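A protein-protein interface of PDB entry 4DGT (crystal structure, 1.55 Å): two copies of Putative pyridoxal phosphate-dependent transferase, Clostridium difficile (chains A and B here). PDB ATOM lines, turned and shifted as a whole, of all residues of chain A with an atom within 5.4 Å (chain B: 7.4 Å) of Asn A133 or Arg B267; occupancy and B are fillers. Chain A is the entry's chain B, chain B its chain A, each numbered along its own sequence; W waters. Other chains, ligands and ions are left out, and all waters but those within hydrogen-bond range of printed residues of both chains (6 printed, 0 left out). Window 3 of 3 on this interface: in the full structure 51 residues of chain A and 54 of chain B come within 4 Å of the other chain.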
ATOM      1  N   SER A 104      14.046  16.534 -18.399  1.00  0.00           N
ATOM      2  CA  SER A 104      13.052  16.152 -17.399  1.00  0.00           C
ATOM      3  C   SER A 104      11.758  16.909 -17.648  1.00  0.00           C
ATOM      4  O   SER A 104      10.686  16.338 -17.619  1.00  0.00           O
ATOM      5  CB  SER A 104      13.574  16.425 -16.025  1.00  0.00           C
ATOM      6  OG  SER A 104      12.636  15.963 -15.034  1.00  0.00           O
ATOM      7  N   ASN A 128      18.431   7.054 -18.149  1.00  0.00           N
ATOM      8  CA  ASN A 128      17.575   6.006 -17.569  1.00  0.00           C
ATOM      9  C   ASN A 128      16.782   6.569 -16.428  1.00  0.00           C
ATOM     10  O   ASN A 128      15.565   6.479 -16.398  1.00  0.00           O
ATOM     11  CB  ASN A 128      18.505   4.831 -17.184  1.00  0.00           C
ATOM     12  CG  ASN A 128      17.793   3.617 -16.652  1.00  0.00           C
ATOM     13  OD1 ASN A 128      16.970   3.737 -15.761  1.00  0.00           O
ATOM     14  ND2 ASN A 128      18.104   2.436 -17.198  1.00  0.00           N
ATOM     15  N   SER A 129      17.446   7.226 -15.495  1.00  0.00           N
ATOM     16  CA  SER A 129      16.744   7.684 -14.293  1.00  0.00           C
ATOM     17  C   SER A 129      15.783   8.827 -14.558  1.00  0.00           C
ATOM     18  O   SER A 129      14.750   8.901 -13.874  1.00  0.00           O
ATOM     19  CB  SER A 129      17.733   8.033 -13.193  1.00  0.00           C
ATOM     20  OG  SER A 129      18.648   9.006 -13.658  1.00  0.00           O
ATOM     21  N   VAL A 130      16.033   9.683 -15.535  1.00  0.00           N
ATOM     22  CA  VAL A 130      15.095  10.820 -15.832  1.00  0.00           C
ATOM     23  C   VAL A 130      13.775  10.322 -16.314  1.00  0.00           C
ATOM     24  O   VAL A 130      12.710  10.843 -15.951  1.00  0.00           O
ATOM     25  CB  VAL A 130      15.722  11.917 -16.745  1.00  0.00           C
ATOM     26  CG1 VAL A 130      15.839  11.448 -18.174  1.00  0.00           C
ATOM     27  CG2 VAL A 130      14.900  13.241 -16.622  1.00  0.00           C
ATOM     28  N   VAL A 131      13.792   9.206 -17.051  1.00  0.00           N
ATOM     29  CA  VAL A 131      12.539   8.626 -17.510  1.00  0.00           C
ATOM     30  C   VAL A 131      11.833   7.983 -16.300  1.00  0.00           C
ATOM     31  O   VAL A 131      10.652   8.237 -16.087  1.00  0.00           O
ATOM     32  CB  VAL A 131      12.798   7.604 -18.618  1.00  0.00           C
ATOM     33  CG1 VAL A 131      11.527   6.847 -19.008  1.00  0.00           C
ATOM     34  CG2 VAL A 131      13.401   8.356 -19.810  1.00  0.00           C
ATOM     35  N   LYS A 132      12.524   7.159 -15.519  1.00  0.00           N
ATOM     36  CA  LYS A 132      11.882   6.440 -14.447  1.00  0.00           C
ATOM     37  C   LYS A 132      11.425   7.390 -13.319  1.00  0.00           C
ATOM     38  O   LYS A 132      10.335   7.225 -12.760  1.00  0.00           O
ATOM     39  CB  LYS A 132      12.787   5.346 -13.869  1.00  0.00           C
ATOM     40  CG  LYS A 132      13.196   4.215 -14.829  1.00  0.00           C
ATOM     41  CD  LYS A 132      12.074   3.559 -15.641  1.00  0.00           C
ATOM     42  CE  LYS A 132      11.069   2.646 -14.929  1.00  0.00           C
ATOM     43  NZ  LYS A 132      11.696   1.382 -14.407  1.00  0.00           N
ATOM     44  N   ASN A 133      12.241   8.397 -12.956  1.00  0.00           N
ATOM     45  CA  ASN A 133      11.860   9.366 -11.944  1.00  0.00           C
ATOM     46  C   ASN A 133      10.659  10.229 -12.331  1.00  0.00           C
ATOM     47  O   ASN A 133      10.040  10.881 -11.469  1.00  0.00           O
ATOM     48  CB  ASN A 133      13.079  10.250 -11.622  1.00  0.00           C
ATOM     49  CG  ASN A 133      14.176   9.460 -10.911  1.00  0.00           C
ATOM     50  OD1 ASN A 133      13.879   8.439 -10.272  1.00  0.00           O
ATOM     51  ND2 ASN A 133      15.415   9.972 -10.957  1.00  0.00           N
ATOM     52  N   ASN A 134      10.353  10.289 -13.617  1.00  0.00           N
ATOM     53  CA  ASN A 134       9.139  10.910 -14.117  1.00  0.00           C
ATOM     54  C   ASN A 134       7.980   9.956 -14.294  1.00  0.00           C
ATOM     55  O   ASN A 134       6.911  10.329 -14.811  1.00  0.00           O
ATOM     56  CB  ASN A 134       9.420  11.696 -15.428  1.00  0.00           C
ATOM     57  CG  ASN A 134      10.001  13.067 -15.156  1.00  0.00           C
ATOM     58  OD1 ASN A 134       9.277  13.935 -14.725  1.00  0.00           O
ATOM     59  ND2 ASN A 134      11.283  13.265 -15.448  1.00  0.00           N
ATOM     60  N   ASN A 135       8.117   8.716 -13.826  1.00  0.00           N
ATOM     61  CA  ASN A 135       7.052   7.740 -13.984  1.00  0.00           C
ATOM     62  C   ASN A 135       6.615   7.555 -15.419  1.00  0.00           C
ATOM     63  O   ASN A 135       5.428   7.407 -15.716  1.00  0.00           O
ATOM     64  CB  ASN A 135       5.896   8.148 -13.105  1.00  0.00           C
ATOM     65  CG  ASN A 135       4.938   7.006 -12.790  1.00  0.00           C
ATOM     66  OD1 ASN A 135       5.272   5.808 -12.907  1.00  0.00           O
ATOM     67  ND2 ASN A 135       3.699   7.378 -12.501  1.00  0.00           N
ATOM     68  N   ARG A 267       6.482  27.523 -14.707  1.00  0.00           N
ATOM     69  CA  ARG A 267       5.920  26.784 -13.583  1.00  0.00           C
ATOM     70  C   ARG A 267       6.892  26.607 -12.431  1.00  0.00           C
ATOM     71  O   ARG A 267       6.504  26.737 -11.228  1.00  0.00           O
ATOM     72  CB  ARG A 267       5.376  25.434 -14.053  1.00  0.00           C
ATOM     73  CG  ARG A 267       4.970  24.453 -12.938  1.00  0.00           C
ATOM     74  CD  ARG A 267       4.368  23.167 -13.452  1.00  0.00           C
ATOM     75  NE  ARG A 267       5.075  22.485 -14.527  1.00  0.00           N
ATOM     76  CZ  ARG A 267       6.042  21.615 -14.389  1.00  0.00           C
ATOM     77  NH1 ARG A 267       6.582  21.382 -13.177  1.00  0.00           N
ATOM     78  NH2 ARG A 267       6.523  20.998 -15.480  1.00  0.00           N
ATOM     79  N   SER B 104       7.192  25.599  -5.821  1.00  0.00           N
ATOM     80  CA  SER B 104       6.544  24.947  -6.927  1.00  0.00           C
ATOM     81  C   SER B 104       6.590  23.436  -6.778  1.00  0.00           C
ATOM     82  O   SER B 104       5.593  22.756  -6.970  1.00  0.00           O
ATOM     83  CB  SER B 104       7.147  25.411  -8.277  1.00  0.00           C
ATOM     84  OG  SER B 104       6.495  24.827  -9.388  1.00  0.00           O
ATOM     85  N   LEU B 105       7.785  22.903  -6.524  1.00  0.00           N
ATOM     86  CA  LEU B 105       7.934  21.491  -6.320  1.00  0.00           C
ATOM     87  C   LEU B 105       7.192  21.004  -5.105  1.00  0.00           C
ATOM     88  O   LEU B 105       6.645  19.921  -5.117  1.00  0.00           O
ATOM     89  CB  LEU B 105       9.444  21.146  -6.238  1.00  0.00           C
ATOM     90  CG  LEU B 105      10.273  21.346  -7.477  1.00  0.00           C
ATOM     91  CD1 LEU B 105      11.701  20.801  -7.240  1.00  0.00           C
ATOM     92  CD2 LEU B 105       9.657  20.686  -8.687  1.00  0.00           C
ATOM     93  N   LEU B 106       7.189  21.809  -4.038  1.00  0.00           N
ATOM     94  CA  LEU B 106       6.461  21.423  -2.832  1.00  0.00           C
ATOM     95  C   LEU B 106       4.959  21.282  -3.144  1.00  0.00           C
ATOM     96  O   LEU B 106       4.314  20.351  -2.670  1.00  0.00           O
ATOM     97  CB  LEU B 106       6.698  22.433  -1.684  1.00  0.00           C
ATOM     98  CG  LEU B 106       8.053  22.396  -1.027  1.00  0.00           C
ATOM     99  CD1 LEU B 106       8.227  23.635  -0.178  1.00  0.00           C
ATOM    100  CD2 LEU B 106       8.163  21.080  -0.205  1.00  0.00           C
ATOM    101  N   ASN B 108       3.611  20.547  -6.023  1.00  0.00           N
ATOM    102  CA  ASN B 108       3.428  19.349  -6.828  1.00  0.00           C
ATOM    103  C   ASN B 108       3.476  18.056  -6.005  1.00  0.00           C
ATOM    104  O   ASN B 108       2.737  17.077  -6.296  1.00  0.00           O
ATOM    105  CB  ASN B 108       4.449  19.272  -7.955  1.00  0.00           C
ATOM    106  CG  ASN B 108       4.147  18.139  -8.919  1.00  0.00           C
ATOM    107  OD1 ASN B 108       3.211  18.239  -9.728  1.00  0.00           O
ATOM    108  ND2 ASN B 108       4.878  17.057  -8.813  1.00  0.00           N
ATOM    109  N   GLU B 109       4.340  18.037  -5.000  1.00  0.00           N
ATOM    110  CA  GLU B 109       4.547  16.843  -4.189  1.00  0.00           C
ATOM    111  C   GLU B 109       3.619  16.674  -3.027  1.00  0.00           C
ATOM    112  O   GLU B 109       3.292  15.496  -2.676  1.00  0.00           O
ATOM    113  CB  GLU B 109       5.976  16.764  -3.691  1.00  0.00           C
ATOM    114  CG  GLU B 109       7.001  16.697  -4.807  1.00  0.00           C
ATOM    115  CD  GLU B 109       6.747  15.559  -5.809  1.00  0.00           C
ATOM    116  OE1 GLU B 109       6.405  14.407  -5.413  1.00  0.00           O
ATOM    117  OE2 GLU B 109       6.828  15.852  -7.031  1.00  0.00           O
ATOM    118  N   LEU B 260      10.158  13.904   0.030  1.00  0.00           N
ATOM    119  CA  LEU B 260       9.379  14.300  -1.152  1.00  0.00           C
ATOM    120  C   LEU B 260      10.054  15.438  -1.912  1.00  0.00           C
ATOM    121  O   LEU B 260      10.143  15.385  -3.134  1.00  0.00           O
ATOM    122  CB  LEU B 260       7.964  14.687  -0.760  1.00  0.00           C
ATOM    123  CG  LEU B 260       7.012  13.512  -0.455  1.00  0.00           C
ATOM    124  CD1 LEU B 260       5.725  14.128   0.113  1.00  0.00           C
ATOM    125  CD2 LEU B 260       6.862  12.690  -1.738  1.00  0.00           C
ATOM    126  N   LEU B 261      10.600  16.434  -1.222  1.00  0.00           N
ATOM    127  CA  LEU B 261      11.246  17.507  -1.952  1.00  0.00           C
ATOM    128  C   LEU B 261      12.607  17.076  -2.526  1.00  0.00           C
ATOM    129  O   LEU B 261      12.939  17.455  -3.644  1.00  0.00           O
ATOM    130  CB  LEU B 261      11.387  18.770  -1.089  1.00  0.00           C
ATOM    131  CG  LEU B 261      11.882  20.014  -1.825  1.00  0.00           C
ATOM    132  CD1 LEU B 261      10.979  20.371  -3.004  1.00  0.00           C
ATOM    133  CD2 LEU B 261      12.001  21.145  -0.816  1.00  0.00           C
ATOM    134  N   ASP B 262      13.375  16.332  -1.755  1.00  0.00           N
ATOM    135  CA  ASP B 262      14.666  15.791  -2.243  1.00  0.00           C
ATOM    136  C   ASP B 262      14.413  14.982  -3.504  1.00  0.00           C
ATOM    137  O   ASP B 262      15.148  15.135  -4.509  1.00  0.00           O
ATOM    138  CB  ASP B 262      15.291  14.928  -1.128  1.00  0.00           C
ATOM    139  CG  ASP B 262      16.767  14.644  -1.320  1.00  0.00           C
ATOM    140  OD1 ASP B 262      17.513  15.465  -1.843  1.00  0.00           O
ATOM    141  OD2 ASP B 262      17.178  13.609  -0.825  1.00  0.00           O
ATOM    142  N   ASP B 263      13.366  14.148  -3.496  1.00  0.00           N
ATOM    143  CA  ASP B 263      13.058  13.354  -4.710  1.00  0.00           C
ATOM    144  C   ASP B 263      12.634  14.207  -5.862  1.00  0.00           C
ATOM    145  O   ASP B 263      13.001  13.889  -6.984  1.00  0.00           O
ATOM    146  CB  ASP B 263      12.004  12.319  -4.393  1.00  0.00           C
ATOM    147  CG  ASP B 263      12.558  11.197  -3.509  1.00  0.00           C
ATOM    148  OD1 ASP B 263      13.797  11.094  -3.356  1.00  0.00           O
ATOM    149  OD2 ASP B 263      11.752  10.408  -3.003  1.00  0.00           O
ATOM    150  N   ALA B 264      11.885  15.283  -5.598  1.00  0.00           N
ATOM    151  CA  ALA B 264      11.482  16.187  -6.664  1.00  0.00           C
ATOM    152  C   ALA B 264      12.712  16.860  -7.286  1.00  0.00           C
ATOM    153  O   ALA B 264      12.790  16.986  -8.494  1.00  0.00           O
ATOM    154  CB  ALA B 264      10.515  17.201  -6.148  1.00  0.00           C
ATOM    155  N   PHE B 265      13.656  17.337  -6.479  1.00  0.00           N
ATOM    156  CA  PHE B 265      14.874  17.947  -7.063  1.00  0.00           C
ATOM    157  C   PHE B 265      15.734  16.908  -7.783  1.00  0.00           C
ATOM    158  O   PHE B 265      16.413  17.271  -8.728  1.00  0.00           O
ATOM    159  CB  PHE B 265      15.675  18.664  -5.979  1.00  0.00           C
ATOM    160  CG  PHE B 265      15.205  20.037  -5.686  1.00  0.00           C
ATOM    161  CD1 PHE B 265      15.308  21.024  -6.617  1.00  0.00           C
ATOM    162  CD2 PHE B 265      14.669  20.362  -4.434  1.00  0.00           C
ATOM    163  CE1 PHE B 265      14.858  22.299  -6.352  1.00  0.00           C
ATOM    164  CE2 PHE B 265      14.258  21.638  -4.144  1.00  0.00           C
ATOM    165  CZ  PHE B 265      14.325  22.597  -5.106  1.00  0.00           C
ATOM    166  N   THR B 266      15.662  15.651  -7.350  1.00  0.00           N
ATOM    167  CA  THR B 266      16.329  14.576  -8.100  1.00  0.00           C
ATOM    168  C   THR B 266      15.677  14.386  -9.445  1.00  0.00           C
ATOM    169  O   THR B 266      16.391  14.258 -10.451  1.00  0.00           O
ATOM    170  CB  THR B 266      16.320  13.273  -7.299  1.00  0.00           C
ATOM    171  OG1 THR B 266      17.188  13.432  -6.145  1.00  0.00           O
ATOM    172  CG2 THR B 266      16.738  12.069  -8.160  1.00  0.00           C
ATOM    173  N   ARG B 267      14.370  14.438  -9.467  1.00  0.00           N
ATOM    174  CA  ARG B 267      13.607  14.276 -10.703  1.00  0.00           C
ATOM    175  C   ARG B 267      13.939  15.319 -11.754  1.00  0.00           C
ATOM    176  O   ARG B 267      14.052  14.992 -12.920  1.00  0.00           O
ATOM    177  CB  ARG B 267      12.113  14.297 -10.430  1.00  0.00           C
ATOM    178  CG  ARG B 267      11.189  14.306 -11.664  1.00  0.00           C
ATOM    179  CD  ARG B 267       9.677  14.362 -11.312  1.00  0.00           C
ATOM    180  NE  ARG B 267       9.234  15.229 -10.231  1.00  0.00           N
ATOM    181  CZ  ARG B 267       8.872  16.510 -10.307  1.00  0.00           C
ATOM    182  NH1 ARG B 267       8.366  17.097  -9.189  1.00  0.00           N
ATOM    183  NH2 ARG B 267       8.965  17.229 -11.450  1.00  0.00           N
ATOM    184  N   ILE B 268      14.128  16.575 -11.361  1.00  0.00           N
ATOM    185  CA  ILE B 268      14.490  17.651 -12.318  1.00  0.00           C
ATOM    186  C   ILE B 268      16.037  17.898 -12.346  1.00  0.00           C
ATOM    187  O   ILE B 268      16.496  18.821 -13.041  1.00  0.00           O
ATOM    188  CB  ILE B 268      13.736  18.959 -12.057  1.00  0.00           C
ATOM    189  CG1 ILE B 268      14.118  19.601 -10.710  1.00  0.00           C
ATOM    190  CG2 ILE B 268      12.203  18.743 -12.093  1.00  0.00           C
ATOM    191  CD1 ILE B 268      13.639  21.058 -10.620  1.00  0.00           C
ATOM    192  N   ASP B 269      16.807  17.114 -11.586  1.00  0.00           N
ATOM    193  CA  ASP B 269      18.272  17.099 -11.543  1.00  0.00           C
ATOM    194  C   ASP B 269      18.831  18.468 -11.211  1.00  0.00           C
ATOM    195  O   ASP B 269      19.783  18.942 -11.834  1.00  0.00           O
ATOM    196  CB  ASP B 269      18.891  16.528 -12.822  1.00  0.00           C
ATOM    197  CG  ASP B 269      20.365  16.288 -12.693  1.00  0.00           C
ATOM    198  OD1 ASP B 269      20.778  15.807 -11.604  1.00  0.00           O
ATOM    199  OD2 ASP B 269      21.112  16.719 -13.627  1.00  0.00           O
ATOM    200  N   ILE B 270      18.277  19.111 -10.195  1.00  0.00           N
ATOM    201  CA  ILE B 270      18.816  20.381  -9.702  1.00  0.00           C
ATOM    202  C   ILE B 270      19.219  20.138  -8.226  1.00  0.00           C
ATOM    203  O   ILE B 270      18.380  20.041  -7.338  1.00  0.00           O
ATOM    204  CB  ILE B 270      17.846  21.551  -9.875  1.00  0.00           C
ATOM    205  CG1 ILE B 270      17.644  21.880 -11.366  1.00  0.00           C
ATOM    206  CG2 ILE B 270      18.330  22.806  -9.098  1.00  0.00           C
ATOM    207  CD1 ILE B 270      16.622  22.916 -11.693  1.00  0.00           C
ATOM    208  N   LYS B 271      20.506  20.003  -8.002  1.00  0.00           N
ATOM    209  CA  LYS B 271      21.076  19.554  -6.759  1.00  0.00           C
ATOM    210  C   LYS B 271      22.240  20.388  -6.266  1.00  0.00           C
ATOM    211  O   LYS B 271      22.472  20.502  -5.065  1.00  0.00           O
ATOM    212  CB  LYS B 271      21.579  18.099  -6.869  1.00  0.00           C
ATOM    213  CG  LYS B 271      20.525  17.059  -7.289  1.00  0.00           C
ATOM    214  CD  LYS B 271      19.342  16.914  -6.352  1.00  0.00           C
ATOM    215  CE  LYS B 271      19.562  16.021  -5.212  1.00  0.00           C
ATOM    216  NZ  LYS B 271      18.277  15.622  -4.566  1.00  0.00           N
HETATM  217  O   HOH W   1       8.056  18.712 -14.067  1.00  0.00           O
HETATM  218  O   HOH W   2       7.127  19.503 -10.416  1.00  0.00           O
HETATM  219  O   HOH W   3       5.828  18.049 -12.513  1.00  0.00           O
HETATM  220  O   HOH W   4      15.908  12.313 -12.635  1.00  0.00           O
HETATM  221  O   HOH W   5       6.143  22.141 -10.366  1.00  0.00           O
HETATM  222  O   HOH W   6       9.921  16.540 -14.158  1.00  0.00           O
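The backbone carbonyl oxygen (O) of Arg B267 sits at hydrogen-bond distance from the side-chain hydroxyl (OG) of Ser A104 (2.7 Å).
The backbone carbonyl oxygen of Arg A267 sits at hydrogen-bond distance from the side-chain hydroxyl of Ser B104 (2.7 Å).
OE2 of Glu B109 lies within salt-bridge range of NH1 of Arg B267.
The side-chain hydroxyl of Thr B266 is in hydrogen-bond range of the backbone carbonyl oxygen of Asp B262 (3.1 Å).
OG1 of Thr B266 is in hydrogen-bond range of NZ of Lys B271, at 2.9 Å.
The backbone carbonyl oxygen (O) of Ser A129 sits close to the side-chain amide nitrogen (ND2) of Asn A133 (3.2 Å).
The side-chain amide nitrogen (ND2) of Asn A134 sits at hydrogen-bond distance from the side-chain hydroxyl (OG) of Ser A104, at 3.0 Å.
The backbone carbonyl oxygen (O) of Val A130 lies within hydrogen-bond range of the side-chain amide nitrogen (ND2) of Asn A134 (2.9 Å).
Ile B268 touches Ser A104 (CA to OG, 3.7 Å).
CG2 of Thr B266 touches ND2 of Asn A133, 3.7 Å away.
O of Asn A133 touches CD of Arg B267 (3.5 Å).
Arg B267 touches Asn A134 (CD to OD1, 3.5 Å).
Asn A133 touches two residues of chain B.
Printed residues of chain B within 4 Å of Arg A267: Ser B104 (2.7 Å).
Of the printed residues of chain B, Ser A104 touches Arg B267 (2.7 Å) and Ile B268 (3.7 Å).
Val A131 touches none of the printed residues of chain B.
The nearest residue of chain B that does not touch Asn A133 is Asp B263 (5.9 Å).
The nearest residue of chain A that does not touch Arg B267 is Val A130 (4.2 Å).
The nearest printed residue of chain A that does not touch Ser B104 is Ser A104 (12.2 Å).
Along chain B the printed residues that touch a printed residue of chain A span positions 104 to 268.
Of the 10 printed residues of chain A, 4 touch a printed residue of chain B.
Among the printed residues, 6 pairs touch across the chains.
Ser A104 touches Arg B267, and with the chains exchanged Arg A267 touches Ser B104.
Of the 6 pairs that touch across the chains among the printed residues, 2 have their exchanged pair printed and touching as well.
Water W6 lies within hydrogen-bond range of OD1 of Asn A134 (2.7 Å), OG of Ser A104 (2.9 Å) and NH2 of Arg B267 (3.0 Å).
Water W5 bridges OG of Ser B104 (2.9 Å) and NH1 of Arg A267 (2.9 Å).
Water W4 lies within hydrogen-bond range of ND2 of Asn A133, O of Thr B266 and O of Arg B267.
Water W2 bridges the guanidinium group of Arg B267 (3.0 Å) and the guanidinium group of Arg A267 (3.4 Å).
Water W1 bridges NH2 of Arg A267 and NH2 of Arg B267.
Water W3 bridges the guanidinium group (NH2) of Arg B267 (3.4 Å) and the guanidinium group (NH1) of Arg A267 (3.5 Å).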
